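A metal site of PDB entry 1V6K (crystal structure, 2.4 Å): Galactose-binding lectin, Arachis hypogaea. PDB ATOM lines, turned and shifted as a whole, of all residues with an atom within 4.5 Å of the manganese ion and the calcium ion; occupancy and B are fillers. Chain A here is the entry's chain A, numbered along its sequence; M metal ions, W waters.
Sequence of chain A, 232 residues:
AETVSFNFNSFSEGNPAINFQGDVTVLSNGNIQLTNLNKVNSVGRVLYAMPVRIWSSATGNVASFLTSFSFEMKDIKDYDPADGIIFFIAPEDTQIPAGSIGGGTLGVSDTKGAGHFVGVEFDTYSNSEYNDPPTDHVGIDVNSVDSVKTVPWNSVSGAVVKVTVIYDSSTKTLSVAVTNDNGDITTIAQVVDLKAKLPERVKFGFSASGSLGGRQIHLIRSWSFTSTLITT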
ATOM      1  N   GLY A 104       0.662 -13.183  21.482  1.00  0.00           N
ATOM      2  CA  GLY A 104       0.100 -12.485  20.334  1.00  0.00           C
ATOM      3  C   GLY A 104       0.751 -12.749  18.991  1.00  0.00           C
ATOM      4  O   GLY A 104       0.253 -12.268  17.973  1.00  0.00           O
ATOM      5  N   GLU A 121      -6.929 -14.713  11.139  1.00  0.00           N
ATOM      6  CA  GLU A 121      -6.855 -14.927  12.572  1.00  0.00           C
ATOM      7  C   GLU A 121      -8.175 -14.758  13.308  1.00  0.00           C
ATOM      8  O   GLU A 121      -9.063 -14.007  12.891  1.00  0.00           O
ATOM      9  CB  GLU A 121      -5.817 -13.996  13.185  1.00  0.00           C
ATOM     10  CG  GLU A 121      -6.085 -12.533  12.910  1.00  0.00           C
ATOM     11  CD  GLU A 121      -5.206 -11.644  13.715  1.00  0.00           C
ATOM     12  OE1 GLU A 121      -3.969 -11.760  13.619  1.00  0.00           O
ATOM     13  OE2 GLU A 121      -5.745 -10.812  14.464  1.00  0.00           O
ATOM     14  N   ASP A 123      -8.521 -13.850  16.763  1.00  0.00           N
ATOM     15  CA  ASP A 123      -7.834 -13.258  17.879  1.00  0.00           C
ATOM     16  C   ASP A 123      -8.697 -12.974  19.084  1.00  0.00           C
ATOM     17  O   ASP A 123      -9.679 -12.257  18.982  1.00  0.00           O
ATOM     18  CB  ASP A 123      -7.198 -11.966  17.402  1.00  0.00           C
ATOM     19  CG  ASP A 123      -5.938 -11.669  18.119  1.00  0.00           C
ATOM     20  OD1 ASP A 123      -5.888 -11.923  19.344  1.00  0.00           O
ATOM     21  OD2 ASP A 123      -5.000 -11.184  17.467  1.00  0.00           O
ATOM     22  N   TYR A 125      -7.293 -11.858  22.232  1.00  0.00           N
ATOM     23  CA  TYR A 125      -6.625 -11.000  23.195  1.00  0.00           C
ATOM     24  C   TYR A 125      -6.083  -9.778  22.477  1.00  0.00           C
ATOM     25  O   TYR A 125      -5.521  -9.887  21.398  1.00  0.00           O
ATOM     26  CB  TYR A 125      -5.486 -11.724  23.901  1.00  0.00           C
ATOM     27  CG  TYR A 125      -4.808 -10.844  24.921  1.00  0.00           C
ATOM     28  CD1 TYR A 125      -3.779  -9.981  24.555  1.00  0.00           C
ATOM     29  CD2 TYR A 125      -5.250 -10.832  26.251  1.00  0.00           C
ATOM     30  CE1 TYR A 125      -3.205  -9.109  25.484  1.00  0.00           C
ATOM     31  CE2 TYR A 125      -4.679  -9.971  27.188  1.00  0.00           C
ATOM     32  CZ  TYR A 125      -3.655  -9.114  26.799  1.00  0.00           C
ATOM     33  OH  TYR A 125      -3.081  -8.271  27.714  1.00  0.00           O
ATOM     34  N   ASN A 127      -3.484  -7.324  21.752  1.00  0.00           N
ATOM     35  CA  ASN A 127      -2.069  -7.001  21.878  1.00  0.00           C
ATOM     36  C   ASN A 127      -1.849  -5.622  21.278  1.00  0.00           C
ATOM     37  O   ASN A 127      -1.850  -5.475  20.054  1.00  0.00           O
ATOM     38  CB  ASN A 127      -1.195  -7.996  21.118  1.00  0.00           C
ATOM     39  CG  ASN A 127      -1.130  -9.342  21.799  1.00  0.00           C
ATOM     40  OD1 ASN A 127      -2.081 -10.106  21.749  1.00  0.00           O
ATOM     41  ND2 ASN A 127      -0.004  -9.633  22.456  1.00  0.00           N
ATOM     42  N   ASP A 132      -3.814  -4.293  17.843  1.00  0.00           N
ATOM     43  CA  ASP A 132      -5.066  -5.033  17.840  1.00  0.00           C
ATOM     44  C   ASP A 132      -6.244  -4.169  18.212  1.00  0.00           C
ATOM     45  O   ASP A 132      -6.115  -3.236  19.006  1.00  0.00           O
ATOM     46  CB  ASP A 132      -5.046  -6.176  18.843  1.00  0.00           C
ATOM     47  CG  ASP A 132      -4.310  -7.377  18.357  1.00  0.00           C
ATOM     48  OD1 ASP A 132      -4.338  -7.654  17.141  1.00  0.00           O
ATOM     49  OD2 ASP A 132      -3.711  -8.068  19.202  1.00  0.00           O
ATOM     50  N   HIS A 137     -11.529 -10.352  17.631  1.00  0.00           N
ATOM     51  CA  HIS A 137     -11.721 -10.001  16.243  1.00  0.00           C
ATOM     52  C   HIS A 137     -11.213 -11.018  15.236  1.00  0.00           C
ATOM     53  O   HIS A 137     -10.451 -11.928  15.570  1.00  0.00           O
ATOM     54  CB  HIS A 137     -11.021  -8.683  15.974  1.00  0.00           C
ATOM     55  CG  HIS A 137      -9.572  -8.699  16.321  1.00  0.00           C
ATOM     56  ND1 HIS A 137      -9.124  -8.607  17.630  1.00  0.00           N
ATOM     57  CD2 HIS A 137      -8.474  -8.873  15.557  1.00  0.00           C
ATOM     58  CE1 HIS A 137      -7.812  -8.716  17.649  1.00  0.00           C
ATOM     59  NE2 HIS A 137      -7.390  -8.880  16.401  1.00  0.00           N
ATOM     60  N   VAL A 145       1.183  -9.885  12.134  1.00  0.00           N
ATOM     61  CA  VAL A 145       0.038 -10.106  12.998  1.00  0.00           C
ATOM     62  C   VAL A 145      -0.649  -8.765  13.243  1.00  0.00           C
ATOM     63  O   VAL A 145      -1.643  -8.676  13.964  1.00  0.00           O
ATOM     64  CB  VAL A 145       0.444 -10.744  14.339  1.00  0.00           C
ATOM     65  CG1 VAL A 145       0.978 -12.132  14.100  1.00  0.00           C
ATOM     66  CG2 VAL A 145       1.459  -9.875  15.053  1.00  0.00           C
ATOM     67  N   SER A 147      -2.792  -6.860  11.657  1.00  0.00           N
ATOM     68  CA  SER A 147      -3.763  -7.003  10.577  1.00  0.00           C
ATOM     69  C   SER A 147      -3.942  -5.866   9.582  1.00  0.00           C
ATOM     70  O   SER A 147      -3.970  -4.685   9.934  1.00  0.00           O
ATOM     71  CB  SER A 147      -5.127  -7.368  11.168  1.00  0.00           C
ATOM     72  OG  SER A 147      -5.067  -8.621  11.837  1.00  0.00           O
HETATM   73 MN    MN M   1      -5.221  -9.444  16.173  1.00  0.00          MN
HETATM   74 CA    CA M   2      -3.704 -10.540  19.774  1.00  0.00          CA
HETATM   75  O   HOH W   1      -5.348  -8.007  14.434  1.00  0.00           O
HETATM   76  O   HOH W   2      -1.915 -10.780  17.897  1.00  0.00           O
HETATM   77  O   HOH W   3      -3.036 -10.039  15.499  1.00  0.00           O
HETATM   78  O   HOH W   4      -3.366 -13.019  20.757  1.00  0.00           O
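Water W3 lies within hydrogen-bond range of the backbone carbonyl oxygen of Val 145 (2.5 Å) and the side-chain carboxylate of Glu 121 (2.7 Å).
The calcium ion is bound by O of Tyr 125 (2.5 Å), OD2 of Asp 132 (2.5 Å), OD1 of Asn 127 (2.6 Å), water W2 (2.6 Å), OD1 of Asp 123 (2.6 Å), water W4 (2.7 Å) and OD2 of Asp 123 (2.7 Å).
The calcium ion has seven donor atoms within binding distance.
Within 4 Å of the calcium ion: Asp 123, Tyr 125, Asn 127 and Asp 132.
The nearest printed residue that does not touch the calcium ion is Gly 104 (4.3 Å).
The manganese ion is bound by OD2 of Asp 123 (2.2 Å), OD1 of Asp 132 (2.2 Å), OE2 of Glu 121 (2.3 Å), NE2 of His 137 (2.3 Å), water W1 (2.3 Å) and water W3 (2.4 Å).
The manganese ion has six donor atoms within binding distance.
The side-chain hydroxyl (OG) of Ser 147 lies close to the side-chain carboxylate (OE2) of Glu 121 (3.5 Å).
Of the 9 residues printed, 4 come within 4 Å of the manganese ion.
The nearest printed residue that does not touch the manganese ion is Val 145 (4.3 Å).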
